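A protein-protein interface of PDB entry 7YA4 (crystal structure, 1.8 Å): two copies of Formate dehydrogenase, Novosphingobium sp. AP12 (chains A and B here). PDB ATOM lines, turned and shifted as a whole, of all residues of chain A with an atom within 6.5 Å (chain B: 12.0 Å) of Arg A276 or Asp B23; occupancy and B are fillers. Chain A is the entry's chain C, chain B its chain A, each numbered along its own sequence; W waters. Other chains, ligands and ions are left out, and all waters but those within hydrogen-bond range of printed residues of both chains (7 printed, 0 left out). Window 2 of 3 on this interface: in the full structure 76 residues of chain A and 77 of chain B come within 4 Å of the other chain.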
ATOM      1  N   TYR A 188       4.498 -10.994  21.015  1.00  0.00           N
ATOM      2  CA  TYR A 188       3.806 -10.672  19.772  1.00  0.00           C
ATOM      3  C   TYR A 188       3.794 -11.885  18.847  1.00  0.00           C
ATOM      4  O   TYR A 188       4.635 -12.753  18.970  1.00  0.00           O
ATOM      5  CB  TYR A 188       4.480  -9.486  19.068  1.00  0.00           C
ATOM      6  CG  TYR A 188       4.462  -8.238  19.903  1.00  0.00           C
ATOM      7  CD1 TYR A 188       3.364  -7.411  19.915  1.00  0.00           C
ATOM      8  CD2 TYR A 188       5.522  -7.946  20.748  1.00  0.00           C
ATOM      9  CE1 TYR A 188       3.327  -6.286  20.732  1.00  0.00           C
ATOM     10  CE2 TYR A 188       5.506  -6.820  21.568  1.00  0.00           C
ATOM     11  CZ  TYR A 188       4.400  -5.979  21.544  1.00  0.00           C
ATOM     12  OH  TYR A 188       4.330  -4.853  22.359  1.00  0.00           O
ATOM     13  N   ASP A 250      10.827  -5.099  11.255  1.00  0.00           N
ATOM     14  CA  ASP A 250      10.586  -5.476  12.650  1.00  0.00           C
ATOM     15  C   ASP A 250      11.658  -6.457  13.138  1.00  0.00           C
ATOM     16  O   ASP A 250      12.004  -6.473  14.306  1.00  0.00           O
ATOM     17  CB  ASP A 250       9.198  -6.099  12.776  1.00  0.00           C
ATOM     18  CG  ASP A 250       8.124  -5.118  12.363  1.00  0.00           C
ATOM     19  OD1 ASP A 250       8.016  -4.094  13.056  1.00  0.00           O
ATOM     20  OD2 ASP A 250       7.465  -5.347  11.332  1.00  0.00           O
ATOM     21  N   MET A 274      16.821   1.883  13.346  1.00  0.00           N
ATOM     22  CA  MET A 274      15.872   0.778  13.390  1.00  0.00           C
ATOM     23  C   MET A 274      14.600   1.205  14.130  1.00  0.00           C
ATOM     24  O   MET A 274      14.586   2.145  14.936  1.00  0.00           O
ATOM     25  CB  MET A 274      16.511  -0.455  14.048  1.00  0.00           C
ATOM     26  CG  MET A 274      17.727  -0.929  13.283  1.00  0.00           C
ATOM     27  SD  MET A 274      18.610  -2.330  14.041  1.00  0.00           S
ATOM     28  CE  MET A 274      17.452  -3.651  13.703  1.00  0.00           C
ATOM     29  N   LYS A 275      13.501   0.536  13.781  1.00  0.00           N
ATOM     30  CA  LYS A 275      12.235   0.697  14.480  1.00  0.00           C
ATOM     31  C   LYS A 275      12.398   0.426  15.975  1.00  0.00           C
ATOM     32  O   LYS A 275      13.120  -0.490  16.365  1.00  0.00           O
ATOM     33  CB  LYS A 275      11.216  -0.291  13.923  1.00  0.00           C
ATOM     34  CG  LYS A 275      10.780  -0.007  12.496  1.00  0.00           C
ATOM     35  CD  LYS A 275       9.698  -0.967  11.977  1.00  0.00           C
ATOM     36  CE  LYS A 275       8.390  -0.809  12.709  1.00  0.00           C
ATOM     37  NZ  LYS A 275       7.327  -1.583  12.012  1.00  0.00           N
ATOM     38  N   ARG A 276      11.690   1.205  16.811  1.00  0.00           N
ATOM     39  CA  ARG A 276      11.695   0.975  18.237  1.00  0.00           C
ATOM     40  C   ARG A 276      11.046  -0.381  18.466  1.00  0.00           C
ATOM     41  O   ARG A 276       9.960  -0.639  17.941  1.00  0.00           O
ATOM     42  CB  ARG A 276      10.924   2.053  19.009  1.00  0.00           C
ATOM     43  CG  ARG A 276      11.082   1.941  20.520  1.00  0.00           C
ATOM     44  CD  ARG A 276      10.370   3.084  21.209  1.00  0.00           C
ATOM     45  NE  ARG A 276       8.939   2.854  21.236  1.00  0.00           N
ATOM     46  CZ  ARG A 276       8.329   2.056  22.106  1.00  0.00           C
ATOM     47  NH1 ARG A 276       9.038   1.414  23.026  1.00  0.00           N
ATOM     48  NH2 ARG A 276       7.026   1.862  22.007  1.00  0.00           N
ATOM     49  N   GLY A 277      11.772  -1.249  19.178  1.00  0.00           N
ATOM     50  CA  GLY A 277      11.290  -2.592  19.470  1.00  0.00           C
ATOM     51  C   GLY A 277      11.684  -3.631  18.423  1.00  0.00           C
ATOM     52  O   GLY A 277      11.067  -4.701  18.369  1.00  0.00           O
ATOM     53  N   ALA A 278      12.636  -3.303  17.540  1.00  0.00           N
ATOM     54  CA  ALA A 278      13.093  -4.226  16.511  1.00  0.00           C
ATOM     55  C   ALA A 278      13.849  -5.370  17.169  1.00  0.00           C
ATOM     56  O   ALA A 278      14.333  -5.222  18.297  1.00  0.00           O
ATOM     57  CB  ALA A 278      13.982  -3.532  15.493  1.00  0.00           C
ATOM     58  N   GLY A 301      15.522  -0.348  25.572  1.00  0.00           N
ATOM     59  CA  GLY A 301      14.267  -0.672  24.919  1.00  0.00           C
ATOM     60  C   GLY A 301      14.217  -0.351  23.434  1.00  0.00           C
ATOM     61  O   GLY A 301      13.216  -0.640  22.789  1.00  0.00           O
ATOM     62  N   HIS A 302      15.306   0.142  22.827  1.00  0.00           N
ATOM     63  CA  HIS A 302      15.256   0.400  21.398  1.00  0.00           C
ATOM     64  C   HIS A 302      15.242  -0.909  20.587  1.00  0.00           C
ATOM     65  O   HIS A 302      14.579  -0.997  19.566  1.00  0.00           O
ATOM     66  CB  HIS A 302      16.393   1.306  20.904  1.00  0.00           C
ATOM     67  CG  HIS A 302      16.034   1.850  19.557  1.00  0.00           C
ATOM     68  ND1 HIS A 302      14.990   2.731  19.374  1.00  0.00           N
ATOM     69  CD2 HIS A 302      16.522   1.563  18.323  1.00  0.00           C
ATOM     70  CE1 HIS A 302      14.860   2.985  18.071  1.00  0.00           C
ATOM     71  NE2 HIS A 302      15.792   2.274  17.410  1.00  0.00           N
ATOM     72  N   LEU A 303      16.008  -1.916  21.017  1.00  0.00           N
ATOM     73  CA  LEU A 303      15.853  -3.276  20.495  1.00  0.00           C
ATOM     74  C   LEU A 303      15.074  -4.079  21.537  1.00  0.00           C
ATOM     75  O   LEU A 303      15.334  -3.955  22.735  1.00  0.00           O
ATOM     76  CB  LEU A 303      17.208  -3.950  20.248  1.00  0.00           C
ATOM     77  CG  LEU A 303      18.083  -3.397  19.124  1.00  0.00           C
ATOM     78  CD1 LEU A 303      19.345  -4.228  19.017  1.00  0.00           C
ATOM     79  CD2 LEU A 303      17.355  -3.319  17.781  1.00  0.00           C
ATOM     80  N   ALA A 304      14.129  -4.893  21.056  1.00  0.00           N
ATOM     81  CA  ALA A 304      13.290  -5.695  21.917  1.00  0.00           C
ATOM     82  C   ALA A 304      13.909  -7.094  22.084  1.00  0.00           C
ATOM     83  O   ALA A 304      13.444  -7.902  22.887  1.00  0.00           O
ATOM     84  CB  ALA A 304      11.887  -5.749  21.353  1.00  0.00           C
ATOM     85  N   PRO B  17       1.441  -2.145  32.668  1.00  0.00           N
ATOM     86  CA  PRO B  17       2.439  -1.363  31.927  1.00  0.00           C
ATOM     87  C   PRO B  17       1.947  -0.004  31.429  1.00  0.00           C
ATOM     88  O   PRO B  17       0.813   0.144  30.952  1.00  0.00           O
ATOM     89  CB  PRO B  17       2.795  -2.269  30.738  1.00  0.00           C
ATOM     90  CG  PRO B  17       1.588  -3.102  30.525  1.00  0.00           C
ATOM     91  CD  PRO B  17       0.998  -3.331  31.908  1.00  0.00           C
ATOM     92  N   LYS B  18       2.831   0.984  31.557  1.00  0.00           N
ATOM     93  CA  LYS B  18       2.585   2.329  31.061  1.00  0.00           C
ATOM     94  C   LYS B  18       3.106   2.501  29.633  1.00  0.00           C
ATOM     95  O   LYS B  18       2.576   3.324  28.902  1.00  0.00           O
ATOM     96  CB  LYS B  18       3.221   3.352  32.013  1.00  0.00           C
ATOM     97  CG  LYS B  18       2.563   3.442  33.384  1.00  0.00           C
ATOM     98  CD  LYS B  18       2.779   4.794  34.063  1.00  0.00           C
ATOM     99  CE  LYS B  18       3.250   4.700  35.505  1.00  0.00           C
ATOM    100  NZ  LYS B  18       2.337   3.912  36.367  1.00  0.00           N
ATOM    101  N   THR B  19       4.120   1.721  29.228  1.00  0.00           N
ATOM    102  CA  THR B  19       4.620   1.708  27.860  1.00  0.00           C
ATOM    103  C   THR B  19       4.764   0.263  27.366  1.00  0.00           C
ATOM    104  O   THR B  19       4.718  -0.665  28.156  1.00  0.00           O
ATOM    105  CB  THR B  19       5.982   2.414  27.751  1.00  0.00           C
ATOM    106  OG1 THR B  19       6.870   1.646  28.552  1.00  0.00           O
ATOM    107  CG2 THR B  19       5.995   3.857  28.224  1.00  0.00           C
ATOM    108  N   TYR B  20       4.863   0.097  26.043  1.00  0.00           N
ATOM    109  CA  TYR B  20       5.029  -1.204  25.406  1.00  0.00           C
ATOM    110  C   TYR B  20       6.336  -1.206  24.615  1.00  0.00           C
ATOM    111  O   TYR B  20       6.941  -0.157  24.437  1.00  0.00           O
ATOM    112  CB  TYR B  20       3.826  -1.466  24.509  1.00  0.00           C
ATOM    113  CG  TYR B  20       2.562  -1.632  25.310  1.00  0.00           C
ATOM    114  CD1 TYR B  20       2.262  -2.833  25.933  1.00  0.00           C
ATOM    115  CD2 TYR B  20       1.771  -0.537  25.611  1.00  0.00           C
ATOM    116  CE1 TYR B  20       1.112  -2.993  26.708  1.00  0.00           C
ATOM    117  CE2 TYR B  20       0.620  -0.676  26.375  1.00  0.00           C
ATOM    118  CZ  TYR B  20       0.292  -1.897  26.931  1.00  0.00           C
ATOM    119  OH  TYR B  20      -0.835  -1.935  27.721  1.00  0.00           O
ATOM    120  N   ALA B  21       6.752  -2.386  24.140  1.00  0.00           N
ATOM    121  CA  ALA B  21       8.040  -2.543  23.498  1.00  0.00           C
ATOM    122  C   ALA B  21       8.047  -1.949  22.095  1.00  0.00           C
ATOM    123  O   ALA B  21       9.132  -1.729  21.564  1.00  0.00           O
ATOM    124  CB  ALA B  21       8.440  -4.006  23.480  1.00  0.00           C
ATOM    125  N   ARG B  22       6.865  -1.736  21.487  1.00  0.00           N
ATOM    126  CA  ARG B  22       6.743  -1.206  20.145  1.00  0.00           C
ATOM    127  C   ARG B  22       5.484  -0.359  20.048  1.00  0.00           C
ATOM    128  O   ARG B  22       4.572  -0.492  20.876  1.00  0.00           O
ATOM    129  CB  ARG B  22       6.625  -2.332  19.121  1.00  0.00           C
ATOM    130  CG  ARG B  22       5.450  -3.247  19.412  1.00  0.00           C
ATOM    131  CD  ARG B  22       5.472  -4.546  18.648  1.00  0.00           C
ATOM    132  NE  ARG B  22       5.260  -4.357  17.227  1.00  0.00           N
ATOM    133  CZ  ARG B  22       6.195  -4.566  16.319  1.00  0.00           C
ATOM    134  NH1 ARG B  22       5.944  -4.279  15.051  1.00  0.00           N
ATOM    135  NH2 ARG B  22       7.354  -5.072  16.703  1.00  0.00           N
ATOM    136  N   ASP B  23       5.427   0.457  18.991  1.00  0.00           N
ATOM    137  CA  ASP B  23       4.399   1.472  18.868  1.00  0.00           C
ATOM    138  C   ASP B  23       3.108   0.946  18.232  1.00  0.00           C
ATOM    139  O   ASP B  23       2.043   1.491  18.496  1.00  0.00           O
ATOM    140  CB  ASP B  23       4.899   2.645  18.033  1.00  0.00           C
ATOM    141  CG  ASP B  23       5.965   3.481  18.710  1.00  0.00           C
ATOM    142  OD1 ASP B  23       6.150   3.369  19.949  1.00  0.00           O
ATOM    143  OD2 ASP B  23       6.625   4.193  17.974  1.00  0.00           O
ATOM    144  N   GLU B  24       3.196  -0.080  17.376  1.00  0.00           N
ATOM    145  CA  GLU B  24       2.048  -0.593  16.647  1.00  0.00           C
ATOM    146  C   GLU B  24       2.227  -2.091  16.393  1.00  0.00           C
ATOM    147  O   GLU B  24       3.352  -2.584  16.388  1.00  0.00           O
ATOM    148  CB  GLU B  24       1.955   0.059  15.267  1.00  0.00           C
ATOM    149  CG  GLU B  24       1.617   1.529  15.299  1.00  0.00           C
ATOM    150  CD  GLU B  24       1.422   2.093  13.902  1.00  0.00           C
ATOM    151  OE1 GLU B  24       0.741   1.428  13.093  1.00  0.00           O
ATOM    152  OE2 GLU B  24       1.946   3.194  13.624  1.00  0.00           O
ATOM    153  N   ILE B  25       1.118  -2.792  16.164  1.00  0.00           N
ATOM    154  CA  ILE B  25       1.163  -4.180  15.709  1.00  0.00           C
ATOM    155  C   ILE B  25       0.471  -4.262  14.356  1.00  0.00           C
ATOM    156  O   ILE B  25      -0.287  -3.344  14.012  1.00  0.00           O
ATOM    157  CB  ILE B  25       0.545  -5.130  16.749  1.00  0.00           C
ATOM    158  CG1 ILE B  25      -0.951  -4.896  16.950  1.00  0.00           C
ATOM    159  CG2 ILE B  25       1.330  -5.031  18.056  1.00  0.00           C
ATOM    160  CD1 ILE B  25      -1.645  -5.970  17.769  1.00  0.00           C
ATOM    161  N   PRO B  26       0.727  -5.319  13.557  1.00  0.00           N
ATOM    162  CA  PRO B  26       0.042  -5.514  12.283  1.00  0.00           C
ATOM    163  C   PRO B  26      -1.479  -5.550  12.391  1.00  0.00           C
ATOM    164  O   PRO B  26      -2.052  -5.922  13.425  1.00  0.00           O
ATOM    165  CB  PRO B  26       0.597  -6.860  11.806  1.00  0.00           C
ATOM    166  CG  PRO B  26       2.000  -6.918  12.399  1.00  0.00           C
ATOM    167  CD  PRO B  26       1.798  -6.318  13.769  1.00  0.00           C
ATOM    168  N   ASN B  27      -2.113  -5.097  11.305  1.00  0.00           N
ATOM    169  CA  ASN B  27      -3.555  -5.101  11.179  1.00  0.00           C
ATOM    170  C   ASN B  27      -3.989  -6.353  10.399  1.00  0.00           C
ATOM    171  O   ASN B  27      -3.792  -6.417   9.192  1.00  0.00           O
ATOM    172  CB  ASN B  27      -3.989  -3.803  10.484  1.00  0.00           C
ATOM    173  CG  ASN B  27      -5.489  -3.622  10.402  1.00  0.00           C
ATOM    174  OD1 ASN B  27      -6.224  -4.051  11.283  1.00  0.00           O
ATOM    175  ND2 ASN B  27      -5.965  -3.037   9.314  1.00  0.00           N
ATOM    176  N   PHE B  45     -10.088   0.256  22.795  1.00  0.00           N
ATOM    177  CA  PHE B  45      -8.680   0.000  23.061  1.00  0.00           C
ATOM    178  C   PHE B  45      -7.880   0.214  21.776  1.00  0.00           C
ATOM    179  O   PHE B  45      -8.422   0.243  20.664  1.00  0.00           O
ATOM    180  CB  PHE B  45      -8.491  -1.403  23.635  1.00  0.00           C
ATOM    181  CG  PHE B  45      -8.908  -2.461  22.644  1.00  0.00           C
ATOM    182  CD1 PHE B  45      -8.003  -2.935  21.696  1.00  0.00           C
ATOM    183  CD2 PHE B  45     -10.201  -2.975  22.655  1.00  0.00           C
ATOM    184  CE1 PHE B  45      -8.410  -3.881  20.772  1.00  0.00           C
ATOM    185  CE2 PHE B  45     -10.594  -3.946  21.740  1.00  0.00           C
ATOM    186  CZ  PHE B  45      -9.700  -4.389  20.800  1.00  0.00           C
ATOM    187  N   LYS B  46      -6.568   0.373  21.940  1.00  0.00           N
ATOM    188  CA  LYS B  46      -5.646   0.382  20.811  1.00  0.00           C
ATOM    189  C   LYS B  46      -5.025  -1.017  20.688  1.00  0.00           C
ATOM    190  O   LYS B  46      -4.468  -1.548  21.659  1.00  0.00           O
ATOM    191  CB  LYS B  46      -4.583   1.469  21.004  1.00  0.00           C
ATOM    192  CG  LYS B  46      -3.612   1.587  19.833  1.00  0.00           C
ATOM    193  CD  LYS B  46      -2.671   2.791  19.839  1.00  0.00           C
ATOM    194  CE  LYS B  46      -1.387   2.506  19.080  1.00  0.00           C
ATOM    195  NZ  LYS B  46      -0.774   3.758  18.577  1.00  0.00           N
ATOM    196  N   PRO B  47      -5.143  -1.692  19.533  1.00  0.00           N
ATOM    197  CA  PRO B  47      -4.472  -2.987  19.352  1.00  0.00           C
ATOM    198  C   PRO B  47      -2.992  -2.926  19.755  1.00  0.00           C
ATOM    199  O   PRO B  47      -2.271  -1.992  19.394  1.00  0.00           O
ATOM    200  CB  PRO B  47      -4.650  -3.273  17.848  1.00  0.00           C
ATOM    201  CG  PRO B  47      -5.934  -2.515  17.472  1.00  0.00           C
ATOM    202  CD  PRO B  47      -5.926  -1.281  18.348  1.00  0.00           C
ATOM    203  N   GLY B  48      -2.585  -3.873  20.596  1.00  0.00           N
ATOM    204  CA  GLY B  48      -1.233  -3.932  21.142  1.00  0.00           C
ATOM    205  C   GLY B  48      -1.183  -3.678  22.644  1.00  0.00           C
ATOM    206  O   GLY B  48      -0.164  -3.954  23.284  1.00  0.00           O
ATOM    207  N   GLU B  49      -2.275  -3.125  23.199  1.00  0.00           N
ATOM    208  CA  GLU B  49      -2.366  -2.927  24.638  1.00  0.00           C
ATOM    209  C   GLU B  49      -2.612  -4.265  25.326  1.00  0.00           C
ATOM    210  O   GLU B  49      -3.083  -5.218  24.694  1.00  0.00           O
ATOM    211  CB  GLU B  49      -3.482  -1.944  25.006  1.00  0.00           C
ATOM    212  CG  GLU B  49      -3.210  -0.513  24.579  1.00  0.00           C
ATOM    213  CD  GLU B  49      -4.301   0.470  24.990  1.00  0.00           C
ATOM    214  OE1 GLU B  49      -3.963   1.417  25.713  1.00  0.00           O
ATOM    215  OE2 GLU B  49      -5.486   0.273  24.630  1.00  0.00           O
ATOM    216  N   LEU B  50      -2.243  -4.322  26.617  1.00  0.00           N
ATOM    217  CA  LEU B  50      -2.503  -5.481  27.463  1.00  0.00           C
ATOM    218  C   LEU B  50      -3.972  -5.494  27.906  1.00  0.00           C
ATOM    219  O   LEU B  50      -4.410  -4.666  28.717  1.00  0.00           O
ATOM    220  CB  LEU B  50      -1.544  -5.489  28.662  1.00  0.00           C
ATOM    221  CG  LEU B  50      -1.767  -6.605  29.657  1.00  0.00           C
ATOM    222  CD1 LEU B  50      -1.540  -7.971  29.003  1.00  0.00           C
ATOM    223  CD2 LEU B  50      -0.838  -6.443  30.844  1.00  0.00           C
ATOM    224  N   LEU B 339      -0.005 -10.248  22.632  1.00  0.00           N
ATOM    225  CA  LEU B 339      -0.723  -8.976  22.538  1.00  0.00           C
ATOM    226  C   LEU B 339      -1.485  -8.906  21.204  1.00  0.00           C
ATOM    227  O   LEU B 339      -2.595  -8.365  21.140  1.00  0.00           O
ATOM    228  CB  LEU B 339       0.255  -7.820  22.733  1.00  0.00           C
ATOM    229  CG  LEU B 339       0.880  -7.763  24.125  1.00  0.00           C
ATOM    230  CD1 LEU B 339       2.083  -6.822  24.156  1.00  0.00           C
ATOM    231  CD2 LEU B 339      -0.192  -7.344  25.110  1.00  0.00           C
ATOM    232  N   SER B 340      -0.907  -9.515  20.155  1.00  0.00           N
ATOM    233  CA  SER B 340      -1.505  -9.607  18.815  1.00  0.00           C
ATOM    234  C   SER B 340      -2.822 -10.399  18.821  1.00  0.00           C
ATOM    235  O   SER B 340      -3.846  -9.982  18.248  1.00  0.00           O
ATOM    236  CB  SER B 340      -0.495 -10.215  17.845  1.00  0.00           C
ATOM    237  OG  SER B 340       0.808  -9.651  18.015  1.00  0.00           O
ATOM    238  N   ALA B 343      -5.694  -8.635  20.721  1.00  0.00           N
ATOM    239  CA  ALA B 343      -6.405  -7.580  19.986  1.00  0.00           C
ATOM    240  C   ALA B 343      -7.618  -8.180  19.281  1.00  0.00           C
ATOM    241  O   ALA B 343      -8.687  -7.571  19.250  1.00  0.00           O
ATOM    242  CB  ALA B 343      -5.491  -6.873  19.021  1.00  0.00           C
HETATM  243  O   HOH W   1       8.674  -5.459  19.493  1.00  0.00           O
HETATM  244  O   HOH W   2       9.953  -5.262  16.073  1.00  0.00           O
HETATM  245  O   HOH W   3       5.316  -4.735  24.785  1.00  0.00           O
HETATM  246  O   HOH W   4       9.031  -2.449  15.879  1.00  0.00           O
HETATM  247  O   HOH W   5      11.334  -2.401  23.001  1.00  0.00           O
HETATM  248  O   HOH W   6       7.820   0.762  17.267  1.00  0.00           O
HETATM  249  O   HOH W   7       2.170  -3.505  21.988  1.00  0.00           O
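O of Ala B21 is in hydrogen-bond range of NH1 of Arg A276 (3.5 Å).
The backbone carbonyl oxygen (O) of Tyr B20 lies within hydrogen-bond range of the guanidinium group (NH1) of Arg A276, 3.0 Å away.
The guanidinium group (NH1) of Arg B22 lies within salt-bridge range of the side-chain carboxylate (OD1) of Asp A250, 2.9 Å away.
OD1 of Asp B23 is in salt-bridge range of NH2 of Arg A276 (2.7 Å).
The guanidinium group of Arg B22 lies within hydrogen-bond range of the backbone carbonyl oxygen of Glu B24, at 2.7 Å.
OH of Tyr B20 lies within hydrogen-bond range of N of Leu B50 (3.0 Å).
The backbone carbonyl oxygen of His A302 is in hydrogen-bond range of the backbone NH of Gly A277, at 2.8 Å.
The side-chain amino group of Lys A275 lies within salt-bridge range of the side-chain carboxylate of Asp A250, at 2.8 Å.
OH of Tyr A188 touches N of Ala B21, at 3.9 Å.
Tyr A188 touches Arg B22.
Tyr A188 touches Ile B25.
OH of Tyr A188 touches CD1 of Leu B339, at 3.5 Å.
CA of Tyr A188 touches OG of Ser B340, at 3.6 Å.
Arg B22 touches Arg A276 (C to NH2, 3.3 Å).
Ala B21 touches Gly A277.
Arg A276 touches just these residues of chain B: Tyr B20 (3.0 Å), Ala B21 (3.5 Å), Arg B22 (3.3 Å) and Asp B23 (2.7 Å).
Of chain A, only Arg A276 (2.7 Å) comes within 4 Å of Asp B23.
No residue of chain B comes within 4 Å of Lys A275.
Gly A277 touches just one residue of chain B: Ala B21 (3.1 Å).
No residue of chain B comes within 4 Å of Ala A278.
No residue of chain B comes within 4 Å of Gly A301.
Of the printed residues of chain B, Asp A250 touches Arg B22 (2.9 Å).
Of the printed residues of chain A, Ser B340 touches Tyr A188.
Printed residues of chain A within 4 Å of Ile B25: Tyr A188 (3.6 Å).
Ala A304 touches none of the printed residues of chain B.
Met A274 touches none of the printed residues of chain B.
Of the 20 printed residues of chain B, 7 touch a printed residue of chain A.
Printed residues of chain B that touch a printed residue of chain A: Tyr B20, Ala B21, Arg B22, Asp B23, Ile B25, Leu B339 and Ser B340.
Along chain B the printed residues that touch a printed residue of chain A span positions 20 to 340.
Printed residues of chain A that touch a printed residue of chain B: Tyr A188, Asp A250, Arg A276 and Gly A277.
Hydrophobic or aromatic side chains of chain A that line the printed part of chain B: Tyr A188.
No position is printed for both chains.
Water W7 bridges OH of Tyr A188 (2.6 Å) and O of Gly B48 (2.7 Å).
Water W5 bridges the backbone carbonyl oxygen of Gly A301 (2.6 Å) and the backbone carbonyl oxygen of Ala B21 (2.7 Å).
Water W3 lies within hydrogen-bond range of OH of Tyr A188 (2.6 Å) and N of Ala B21 (2.8 Å).
Water W6 bridges the backbone carbonyl oxygen (O) of Arg A276 (2.6 Å) and the backbone NH (N) of Asp B23 (3.0 Å).
Water W1 bridges O of Gly A277 (2.8 Å) and NH2 of Arg B22 (3.1 Å).
Water W4 lies within hydrogen-bond range of O of Arg A276 (2.9 Å), NH2 of Arg B22 (3.2 Å) and OD1 of Asp A250 (3.4 Å).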
